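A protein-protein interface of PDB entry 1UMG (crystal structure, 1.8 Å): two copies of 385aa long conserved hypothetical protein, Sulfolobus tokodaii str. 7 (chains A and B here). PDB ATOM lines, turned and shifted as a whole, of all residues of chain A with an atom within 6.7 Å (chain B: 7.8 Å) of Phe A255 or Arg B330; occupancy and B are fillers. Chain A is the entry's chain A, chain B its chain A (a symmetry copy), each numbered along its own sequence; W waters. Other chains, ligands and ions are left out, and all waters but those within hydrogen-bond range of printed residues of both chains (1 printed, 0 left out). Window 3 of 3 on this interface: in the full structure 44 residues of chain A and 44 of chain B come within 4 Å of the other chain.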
ATOM      1  N   LEU A 139      19.299 -19.743  21.446  1.00  0.00           N
ATOM      2  CA  LEU A 139      19.956 -18.521  21.897  1.00  0.00           C
ATOM      3  C   LEU A 139      19.038 -17.300  21.776  1.00  0.00           C
ATOM      4  O   LEU A 139      18.891 -16.536  22.726  1.00  0.00           O
ATOM      5  CB  LEU A 139      21.262 -18.302  21.119  1.00  0.00           C
ATOM      6  CG  LEU A 139      22.038 -16.998  21.339  1.00  0.00           C
ATOM      7  CD1 LEU A 139      22.155 -16.689  22.820  1.00  0.00           C
ATOM      8  CD2 LEU A 139      23.425 -17.134  20.711  1.00  0.00           C
ATOM      9  N   PRO A 140      18.410 -17.099  20.605  1.00  0.00           N
ATOM     10  CA  PRO A 140      17.512 -15.949  20.432  1.00  0.00           C
ATOM     11  C   PRO A 140      16.362 -15.925  21.449  1.00  0.00           C
ATOM     12  O   PRO A 140      16.071 -14.889  22.049  1.00  0.00           O
ATOM     13  CB  PRO A 140      17.011 -16.120  19.004  1.00  0.00           C
ATOM     14  CG  PRO A 140      18.193 -16.737  18.315  1.00  0.00           C
ATOM     15  CD  PRO A 140      18.657 -17.770  19.312  1.00  0.00           C
ATOM     16  N   LYS A 143      17.453 -15.011  24.930  1.00  0.00           N
ATOM     17  CA  LYS A 143      17.663 -13.575  25.028  1.00  0.00           C
ATOM     18  C   LYS A 143      16.347 -12.809  25.088  1.00  0.00           C
ATOM     19  O   LYS A 143      16.167 -11.946  25.945  1.00  0.00           O
ATOM     20  CB  LYS A 143      18.528 -13.082  23.860  1.00  0.00           C
ATOM     21  CG  LYS A 143      19.991 -13.492  24.018  1.00  0.00           C
ATOM     22  CD  LYS A 143      20.925 -12.800  23.033  1.00  0.00           C
ATOM     23  CE  LYS A 143      20.778 -13.330  21.622  1.00  0.00           C
ATOM     24  NZ  LYS A 143      21.877 -12.796  20.757  1.00  0.00           N
ATOM     25  N   LEU A 250      13.545  -8.544  17.938  1.00  0.00           N
ATOM     26  CA  LEU A 250      14.513  -8.323  16.867  1.00  0.00           C
ATOM     27  C   LEU A 250      15.925  -8.115  17.408  1.00  0.00           C
ATOM     28  O   LEU A 250      16.905  -8.432  16.733  1.00  0.00           O
ATOM     29  CB  LEU A 250      14.104  -7.122  16.006  1.00  0.00           C
ATOM     30  CG  LEU A 250      12.817  -7.304  15.198  1.00  0.00           C
ATOM     31  CD1 LEU A 250      12.540  -6.050  14.376  1.00  0.00           C
ATOM     32  CD2 LEU A 250      12.952  -8.517  14.285  1.00  0.00           C
ATOM     33  N   GLU A 251      16.022  -7.582  18.622  1.00  0.00           N
ATOM     34  CA  GLU A 251      17.316  -7.354  19.247  1.00  0.00           C
ATOM     35  C   GLU A 251      18.026  -8.703  19.424  1.00  0.00           C
ATOM     36  O   GLU A 251      19.255  -8.786  19.338  1.00  0.00           O
ATOM     37  CB  GLU A 251      17.124  -6.679  20.612  1.00  0.00           C
ATOM     38  CG  GLU A 251      18.417  -6.434  21.387  1.00  0.00           C
ATOM     39  CD  GLU A 251      19.327  -5.411  20.724  1.00  0.00           C
ATOM     40  OE1 GLU A 251      20.510  -5.341  21.114  1.00  0.00           O
ATOM     41  OE2 GLU A 251      18.863  -4.672  19.828  1.00  0.00           O
ATOM     42  N   ALA A 252      17.243  -9.756  19.649  1.00  0.00           N
ATOM     43  CA  ALA A 252      17.793 -11.097  19.855  1.00  0.00           C
ATOM     44  C   ALA A 252      18.412 -11.707  18.600  1.00  0.00           C
ATOM     45  O   ALA A 252      19.079 -12.742  18.667  1.00  0.00           O
ATOM     46  CB  ALA A 252      16.711 -12.034  20.418  1.00  0.00           C
ATOM     47  N   PHE A 253      18.194 -11.071  17.455  1.00  0.00           N
ATOM     48  CA  PHE A 253      18.753 -11.553  16.201  1.00  0.00           C
ATOM     49  C   PHE A 253      19.784 -10.574  15.641  1.00  0.00           C
ATOM     50  O   PHE A 253      20.321 -10.795  14.553  1.00  0.00           O
ATOM     51  CB  PHE A 253      17.640 -11.770  15.171  1.00  0.00           C
ATOM     52  CG  PHE A 253      16.787 -12.981  15.440  1.00  0.00           C
ATOM     53  CD1 PHE A 253      17.325 -14.262  15.347  1.00  0.00           C
ATOM     54  CD2 PHE A 253      15.443 -12.842  15.776  1.00  0.00           C
ATOM     55  CE1 PHE A 253      16.532 -15.386  15.574  1.00  0.00           C
ATOM     56  CE2 PHE A 253      14.645 -13.957  16.005  1.00  0.00           C
ATOM     57  CZ  PHE A 253      15.189 -15.234  15.906  1.00  0.00           C
ATOM     58  N   ALA A 254      20.062  -9.502  16.381  1.00  0.00           N
ATOM     59  CA  ALA A 254      21.030  -8.495  15.936  1.00  0.00           C
ATOM     60  C   ALA A 254      22.431  -9.087  15.843  1.00  0.00           C
ATOM     61  O   ALA A 254      23.278  -8.605  15.083  1.00  0.00           O
ATOM     62  CB  ALA A 254      21.022  -7.303  16.885  1.00  0.00           C
ATOM     63  N   PHE A 255      22.667 -10.132  16.629  1.00  0.00           N
ATOM     64  CA  PHE A 255      23.946 -10.827  16.634  1.00  0.00           C
ATOM     65  C   PHE A 255      23.784 -12.079  15.782  1.00  0.00           C
ATOM     66  O   PHE A 255      22.990 -12.958  16.114  1.00  0.00           O
ATOM     67  CB  PHE A 255      24.329 -11.236  18.058  1.00  0.00           C
ATOM     68  CG  PHE A 255      25.584 -12.054  18.131  1.00  0.00           C
ATOM     69  CD1 PHE A 255      26.814 -11.489  17.809  1.00  0.00           C
ATOM     70  CD2 PHE A 255      25.536 -13.398  18.493  1.00  0.00           C
ATOM     71  CE1 PHE A 255      27.979 -12.250  17.842  1.00  0.00           C
ATOM     72  CE2 PHE A 255      26.701 -14.171  18.530  1.00  0.00           C
ATOM     73  CZ  PHE A 255      27.922 -13.593  18.201  1.00  0.00           C
ATOM     74  N   PRO A 256      24.531 -12.179  14.671  1.00  0.00           N
ATOM     75  CA  PRO A 256      24.434 -13.350  13.794  1.00  0.00           C
ATOM     76  C   PRO A 256      25.232 -14.515  14.375  1.00  0.00           C
ATOM     77  O   PRO A 256      26.368 -14.761  13.976  1.00  0.00           O
ATOM     78  CB  PRO A 256      25.016 -12.835  12.483  1.00  0.00           C
ATOM     79  CG  PRO A 256      26.135 -11.940  12.965  1.00  0.00           C
ATOM     80  CD  PRO A 256      25.517 -11.206  14.155  1.00  0.00           C
ATOM     81  N   HIS A 257      24.624 -15.240  15.314  1.00  0.00           N
ATOM     82  CA  HIS A 257      25.301 -16.352  15.966  1.00  0.00           C
ATOM     83  C   HIS A 257      25.504 -17.558  15.061  1.00  0.00           C
ATOM     84  O   HIS A 257      24.808 -17.730  14.058  1.00  0.00           O
ATOM     85  CB  HIS A 257      24.544 -16.767  17.241  1.00  0.00           C
ATOM     86  CG  HIS A 257      23.173 -17.322  16.991  1.00  0.00           C
ATOM     87  ND1 HIS A 257      22.171 -16.594  16.388  1.00  0.00           N
ATOM     88  CD2 HIS A 257      22.632 -18.524  17.299  1.00  0.00           C
ATOM     89  CE1 HIS A 257      21.070 -17.326  16.335  1.00  0.00           C
ATOM     90  NE2 HIS A 257      21.323 -18.500  16.880  1.00  0.00           N
ATOM     91  N   LEU A 258      26.487 -18.382  15.414  1.00  0.00           N
ATOM     92  CA  LEU A 258      26.791 -19.579  14.646  1.00  0.00           C
ATOM     93  C   LEU A 258      25.738 -20.636  14.929  1.00  0.00           C
ATOM     94  O   LEU A 258      25.467 -20.952  16.090  1.00  0.00           O
ATOM     95  CB  LEU A 258      28.167 -20.124  15.032  1.00  0.00           C
ATOM     96  CG  LEU A 258      29.366 -19.251  14.657  1.00  0.00           C
ATOM     97  CD1 LEU A 258      30.647 -19.865  15.240  1.00  0.00           C
ATOM     98  CD2 LEU A 258      29.455 -19.149  13.140  1.00  0.00           C
ATOM     99  N   LEU A 271      24.019 -17.140  11.335  1.00  0.00           N
ATOM    100  CA  LEU A 271      22.635 -16.943  10.925  1.00  0.00           C
ATOM    101  C   LEU A 271      22.545 -15.525  10.366  1.00  0.00           C
ATOM    102  O   LEU A 271      22.846 -14.555  11.057  1.00  0.00           O
ATOM    103  CB  LEU A 271      21.690 -17.109  12.120  1.00  0.00           C
ATOM    104  CG  LEU A 271      20.197 -17.087  11.772  1.00  0.00           C
ATOM    105  CD1 LEU A 271      19.888 -18.194  10.772  1.00  0.00           C
ATOM    106  CD2 LEU A 271      19.375 -17.265  13.038  1.00  0.00           C
ATOM    107  N   PRO A 273      20.185 -12.619   9.009  1.00  0.00           N
ATOM    108  CA  PRO A 273      18.821 -12.083   8.889  1.00  0.00           C
ATOM    109  C   PRO A 273      18.743 -11.337   7.560  1.00  0.00           C
ATOM    110  O   PRO A 273      19.561 -10.451   7.300  1.00  0.00           O
ATOM    111  CB  PRO A 273      18.708 -11.132  10.082  1.00  0.00           C
ATOM    112  CG  PRO A 273      19.768 -11.628  11.046  1.00  0.00           C
ATOM    113  CD  PRO A 273      20.901 -11.958  10.111  1.00  0.00           C
ATOM    114  N   THR A 317      24.738  -6.349  10.801  1.00  0.00           N
ATOM    115  CA  THR A 317      24.534  -7.729  11.219  1.00  0.00           C
ATOM    116  C   THR A 317      24.899  -8.620  10.031  1.00  0.00           C
ATOM    117  O   THR A 317      25.615  -9.614  10.179  1.00  0.00           O
ATOM    118  CB  THR A 317      23.067  -7.978  11.612  1.00  0.00           C
ATOM    119  OG1 THR A 317      22.720  -7.122  12.709  1.00  0.00           O
ATOM    120  CG2 THR A 317      22.859  -9.427  12.018  1.00  0.00           C
ATOM    121  N   LEU A 320      28.682  -8.558   9.233  1.00  0.00           N
ATOM    122  CA  LEU A 320      29.406  -9.402  10.179  1.00  0.00           C
ATOM    123  C   LEU A 320      29.195 -10.866   9.801  1.00  0.00           C
ATOM    124  O   LEU A 320      30.114 -11.684   9.896  1.00  0.00           O
ATOM    125  CB  LEU A 320      28.919  -9.148  11.616  1.00  0.00           C
ATOM    126  CG  LEU A 320      29.569 -10.015  12.703  1.00  0.00           C
ATOM    127  CD1 LEU A 320      31.084  -9.832  12.680  1.00  0.00           C
ATOM    128  CD2 LEU A 320      29.009  -9.638  14.076  1.00  0.00           C
ATOM    129  N   ARG B 283      42.367 -12.520  28.836  1.00  0.00           N
ATOM    130  CA  ARG B 283      40.933 -12.480  28.569  1.00  0.00           C
ATOM    131  C   ARG B 283      40.297 -13.863  28.436  1.00  0.00           C
ATOM    132  O   ARG B 283      40.635 -14.627  27.528  1.00  0.00           O
ATOM    133  CB  ARG B 283      40.648 -11.686  27.290  1.00  0.00           C
ATOM    134  CG  ARG B 283      39.165 -11.419  27.125  1.00  0.00           C
ATOM    135  CD  ARG B 283      38.674 -11.561  25.698  1.00  0.00           C
ATOM    136  NE  ARG B 283      37.217 -11.446  25.666  1.00  0.00           N
ATOM    137  CZ  ARG B 283      36.531 -10.806  24.726  1.00  0.00           C
ATOM    138  NH1 ARG B 283      35.207 -10.756  24.789  1.00  0.00           N
ATOM    139  NH2 ARG B 283      37.166 -10.211  23.728  1.00  0.00           N
ATOM    140  N   ILE B 323      39.414 -10.156  17.238  1.00  0.00           N
ATOM    141  CA  ILE B 323      38.085  -9.890  16.688  1.00  0.00           C
ATOM    142  C   ILE B 323      37.215 -11.143  16.779  1.00  0.00           C
ATOM    143  O   ILE B 323      36.057 -11.087  17.197  1.00  0.00           O
ATOM    144  CB  ILE B 323      38.195  -9.429  15.219  1.00  0.00           C
ATOM    145  CG1 ILE B 323      38.868  -8.053  15.183  1.00  0.00           C
ATOM    146  CG2 ILE B 323      36.812  -9.396  14.560  1.00  0.00           C
ATOM    147  CD1 ILE B 323      39.196  -7.553  13.787  1.00  0.00           C
ATOM    148  N   VAL B 324      37.786 -12.276  16.387  1.00  0.00           N
ATOM    149  CA  VAL B 324      37.077 -13.544  16.448  1.00  0.00           C
ATOM    150  C   VAL B 324      36.794 -13.917  17.901  1.00  0.00           C
ATOM    151  O   VAL B 324      35.738 -14.464  18.217  1.00  0.00           O
ATOM    152  CB  VAL B 324      37.901 -14.658  15.758  1.00  0.00           C
ATOM    153  CG1 VAL B 324      37.322 -16.033  16.085  1.00  0.00           C
ATOM    154  CG2 VAL B 324      37.891 -14.432  14.246  1.00  0.00           C
ATOM    155  N   ALA B 325      37.731 -13.613  18.795  1.00  0.00           N
ATOM    156  CA  ALA B 325      37.531 -13.925  20.208  1.00  0.00           C
ATOM    157  C   ALA B 325      36.287 -13.210  20.731  1.00  0.00           C
ATOM    158  O   ALA B 325      35.476 -13.791  21.455  1.00  0.00           O
ATOM    159  CB  ALA B 325      38.749 -13.512  21.014  1.00  0.00           C
ATOM    160  N   ASP B 326      36.132 -11.943  20.362  1.00  0.00           N
ATOM    161  CA  ASP B 326      34.973 -11.181  20.814  1.00  0.00           C
ATOM    162  C   ASP B 326      33.697 -11.777  20.233  1.00  0.00           C
ATOM    163  O   ASP B 326      32.693 -11.947  20.935  1.00  0.00           O
ATOM    164  CB  ASP B 326      35.097  -9.719  20.387  1.00  0.00           C
ATOM    165  CG  ASP B 326      34.167  -8.813  21.163  1.00  0.00           C
ATOM    166  OD1 ASP B 326      34.415  -8.605  22.375  1.00  0.00           O
ATOM    167  OD2 ASP B 326      33.186  -8.318  20.571  1.00  0.00           O
ATOM    168  N   TYR B 327      33.737 -12.101  18.946  1.00  0.00           N
ATOM    169  CA  TYR B 327      32.582 -12.685  18.278  1.00  0.00           C
ATOM    170  C   TYR B 327      32.163 -13.982  18.967  1.00  0.00           C
ATOM    171  O   TYR B 327      30.987 -14.170  19.288  1.00  0.00           O
ATOM    172  CB  TYR B 327      32.902 -12.962  16.809  1.00  0.00           C
ATOM    173  CG  TYR B 327      31.814 -13.715  16.094  1.00  0.00           C
ATOM    174  CD1 TYR B 327      30.605 -13.096  15.765  1.00  0.00           C
ATOM    175  CD2 TYR B 327      31.966 -15.066  15.794  1.00  0.00           C
ATOM    176  CE1 TYR B 327      29.579 -13.809  15.155  1.00  0.00           C
ATOM    177  CE2 TYR B 327      30.953 -15.785  15.189  1.00  0.00           C
ATOM    178  CZ  TYR B 327      29.760 -15.156  14.871  1.00  0.00           C
ATOM    179  OH  TYR B 327      28.757 -15.885  14.278  1.00  0.00           O
ATOM    180  N   MET B 328      33.115 -14.881  19.193  1.00  0.00           N
ATOM    181  CA  MET B 328      32.789 -16.147  19.843  1.00  0.00           C
ATOM    182  C   MET B 328      32.183 -15.931  21.230  1.00  0.00           C
ATOM    183  O   MET B 328      31.195 -16.570  21.588  1.00  0.00           O
ATOM    184  CB  MET B 328      34.037 -17.033  19.964  1.00  0.00           C
ATOM    185  CG  MET B 328      34.646 -17.461  18.631  1.00  0.00           C
ATOM    186  SD  MET B 328      33.529 -18.364  17.544  1.00  0.00           S
ATOM    187  CE  MET B 328      33.354 -19.902  18.465  1.00  0.00           C
ATOM    188  N   ARG B 329      32.774 -15.020  22.000  1.00  0.00           N
ATOM    189  CA  ARG B 329      32.304 -14.740  23.355  1.00  0.00           C
ATOM    190  C   ARG B 329      30.858 -14.262  23.442  1.00  0.00           C
ATOM    191  O   ARG B 329      30.209 -14.432  24.476  1.00  0.00           O
ATOM    192  CB  ARG B 329      33.236 -13.726  24.027  1.00  0.00           C
ATOM    193  CG  ARG B 329      34.609 -14.304  24.365  1.00  0.00           C
ATOM    194  CD  ARG B 329      34.659 -14.939  25.758  1.00  0.00           C
ATOM    195  NE  ARG B 329      33.587 -15.904  26.021  1.00  0.00           N
ATOM    196  CZ  ARG B 329      32.528 -15.665  26.789  1.00  0.00           C
ATOM    197  NH1 ARG B 329      32.383 -14.484  27.383  1.00  0.00           N
ATOM    198  NH2 ARG B 329      31.618 -16.611  26.986  1.00  0.00           N
ATOM    199  N   ARG B 330      30.340 -13.668  22.373  1.00  0.00           N
ATOM    200  CA  ARG B 330      28.958 -13.203  22.410  1.00  0.00           C
ATOM    201  C   ARG B 330      27.970 -14.372  22.399  1.00  0.00           C
ATOM    202  O   ARG B 330      26.763 -14.176  22.563  1.00  0.00           O
ATOM    203  CB  ARG B 330      28.683 -12.242  21.252  1.00  0.00           C
ATOM    204  CG  ARG B 330      29.555 -10.999  21.311  1.00  0.00           C
ATOM    205  CD  ARG B 330      28.979  -9.851  20.505  1.00  0.00           C
ATOM    206  NE  ARG B 330      27.667  -9.462  21.009  1.00  0.00           N
ATOM    207  CZ  ARG B 330      27.026  -8.354  20.650  1.00  0.00           C
ATOM    208  NH1 ARG B 330      27.581  -7.520  19.784  1.00  0.00           N
ATOM    209  NH2 ARG B 330      25.829  -8.090  21.155  1.00  0.00           N
ATOM    210  N   HIS B 331      28.487 -15.587  22.217  1.00  0.00           N
ATOM    211  CA  HIS B 331      27.652 -16.792  22.217  1.00  0.00           C
ATOM    212  C   HIS B 331      27.414 -17.293  23.640  1.00  0.00           C
ATOM    213  O   HIS B 331      26.566 -18.157  23.865  1.00  0.00           O
ATOM    214  CB  HIS B 331      28.304 -17.931  21.429  1.00  0.00           C
ATOM    215  CG  HIS B 331      28.309 -17.732  19.945  1.00  0.00           C
ATOM    216  ND1 HIS B 331      29.182 -16.877  19.314  1.00  0.00           N
ATOM    217  CD2 HIS B 331      27.556 -18.293  18.970  1.00  0.00           C
ATOM    218  CE1 HIS B 331      28.970 -16.923  18.008  1.00  0.00           C
ATOM    219  NE2 HIS B 331      27.989 -17.775  17.777  1.00  0.00           N
ATOM    220  N   GLY B 332      28.177 -16.773  24.592  1.00  0.00           N
ATOM    221  CA  GLY B 332      28.015 -17.215  25.966  1.00  0.00           C
ATOM    222  C   GLY B 332      28.213 -18.717  26.090  1.00  0.00           C
ATOM    223  O   GLY B 332      29.081 -19.282  25.427  1.00  0.00           O
ATOM    224  N   PRO B 333      27.407 -19.398  26.920  1.00  0.00           N
ATOM    225  CA  PRO B 333      27.518 -20.849  27.120  1.00  0.00           C
ATOM    226  C   PRO B 333      26.860 -21.719  26.050  1.00  0.00           C
ATOM    227  O   PRO B 333      26.458 -22.848  26.327  1.00  0.00           O
ATOM    228  CB  PRO B 333      26.878 -21.043  28.492  1.00  0.00           C
ATOM    229  CG  PRO B 333      25.737 -20.068  28.432  1.00  0.00           C
ATOM    230  CD  PRO B 333      26.382 -18.823  27.810  1.00  0.00           C
ATOM    231  N   PHE B 334      26.749 -21.199  24.831  1.00  0.00           N
ATOM    232  CA  PHE B 334      26.140 -21.944  23.729  1.00  0.00           C
ATOM    233  C   PHE B 334      27.159 -22.516  22.751  1.00  0.00           C
ATOM    234  O   PHE B 334      28.187 -21.894  22.486  1.00  0.00           O
ATOM    235  CB  PHE B 334      25.198 -21.032  22.932  1.00  0.00           C
ATOM    236  CG  PHE B 334      23.904 -20.732  23.629  1.00  0.00           C
ATOM    237  CD1 PHE B 334      22.766 -21.484  23.350  1.00  0.00           C
ATOM    238  CD2 PHE B 334      23.820 -19.704  24.562  1.00  0.00           C
ATOM    239  CE1 PHE B 334      21.558 -21.211  23.989  1.00  0.00           C
ATOM    240  CE2 PHE B 334      22.621 -19.423  25.210  1.00  0.00           C
ATOM    241  CZ  PHE B 334      21.486 -20.182  24.922  1.00  0.00           C
ATOM    242  N   HIS B 337      30.520 -22.132  20.576  1.00  0.00           N
ATOM    243  CA  HIS B 337      31.560 -21.492  21.378  1.00  0.00           C
ATOM    244  C   HIS B 337      31.882 -22.448  22.530  1.00  0.00           C
ATOM    245  O   HIS B 337      33.049 -22.681  22.847  1.00  0.00           O
ATOM    246  CB  HIS B 337      31.112 -20.127  21.913  1.00  0.00           C
ATOM    247  CG  HIS B 337      32.101 -19.487  22.834  1.00  0.00           C
ATOM    248  ND1 HIS B 337      33.469 -19.651  22.689  1.00  0.00           N
ATOM    249  CD2 HIS B 337      31.938 -18.687  23.912  1.00  0.00           C
ATOM    250  CE1 HIS B 337      34.097 -18.984  23.639  1.00  0.00           C
ATOM    251  NE2 HIS B 337      33.187 -18.387  24.398  1.00  0.00           N
HETATM  252  O   HOH W   1      24.481 -12.753  22.143  1.00  0.00           O
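O of His A257 sits at hydrogen-bond distance from N of Leu A271 (2.9 Å). O of Tyr B327 is in hydrogen-bond range of ND1 of His B331 (3.3 Å). The backbone carbonyl oxygen of Met B328 lies within hydrogen-bond range of a ring nitrogen (ND1) of His B331, 3.1 Å away.
Among the printed residues, pairs that only touch across the chains: Leu A139 with Phe B334, Phe A255 with Tyr B327, Phe A255 with Arg B330, Phe A255 with His B331, His A257 with Tyr B327, His A257 with His B331, Leu A258 with Tyr B327 and Leu A258 with Met B328.
The backbone carbonyl oxygen (O) of Pro A256 lies within hydrogen-bond range of the side-chain hydroxyl (OH) of Tyr B327, 2.7 Å away. The backbone NH (N) of Leu A258 lies within hydrogen-bond range of a ring nitrogen (NE2) of His B331.
Of the 16 printed residues of chain A, 5 touch a printed residue of chain B. Hydrophobic or aromatic side chains of chain A that line the printed part of chain B: Leu A139, Phe A255, His A257 and Leu A258. Of the 14 printed residues of chain B, 5 touch a printed residue of chain A. Printed residues of chain B that touch a printed residue of chain A: Tyr B327, Met B328, Arg B330, His B331 and Phe B334. Hydrophobic or aromatic side chains of chain B that line the printed part of chain A: Tyr B327, Met B328, His B331 and Phe B334. Along chain B the printed residues that touch a printed residue of chain A span positions 327 to 334. Among the printed residues, no Asp or Glu carboxylate lies within 4 Å of a Lys or Arg side-chain nitrogen of the other chain.
Phe A255 touches three residues of chain B. Of the printed residues of chain A, Arg B330 touches Phe A255 (3.4 Å). No residue of chain B comes within 4 Å of Ala A254. Printed residues of chain A within 4 Å of Tyr B327: Phe A255, Pro A256, His A257 and Leu A258. Of the printed residues of chain B, His A257 touches Tyr B327 (3.7 Å) and His B331 (3.5 Å). Printed residues of chain B within 4 Å of Leu A258: Tyr B327, Met B328 and His B331. The nearest printed residue of chain B that does not touch Leu A258 is His B337 (5.8 Å).
Water W1 lies within hydrogen-bond range of O of Arg B330 and NZ of Lys A143.
No position is printed for both chains. Of the 10 pairs that touch across the chains among the printed residues, none has its exchanged pair printed and touching as well.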
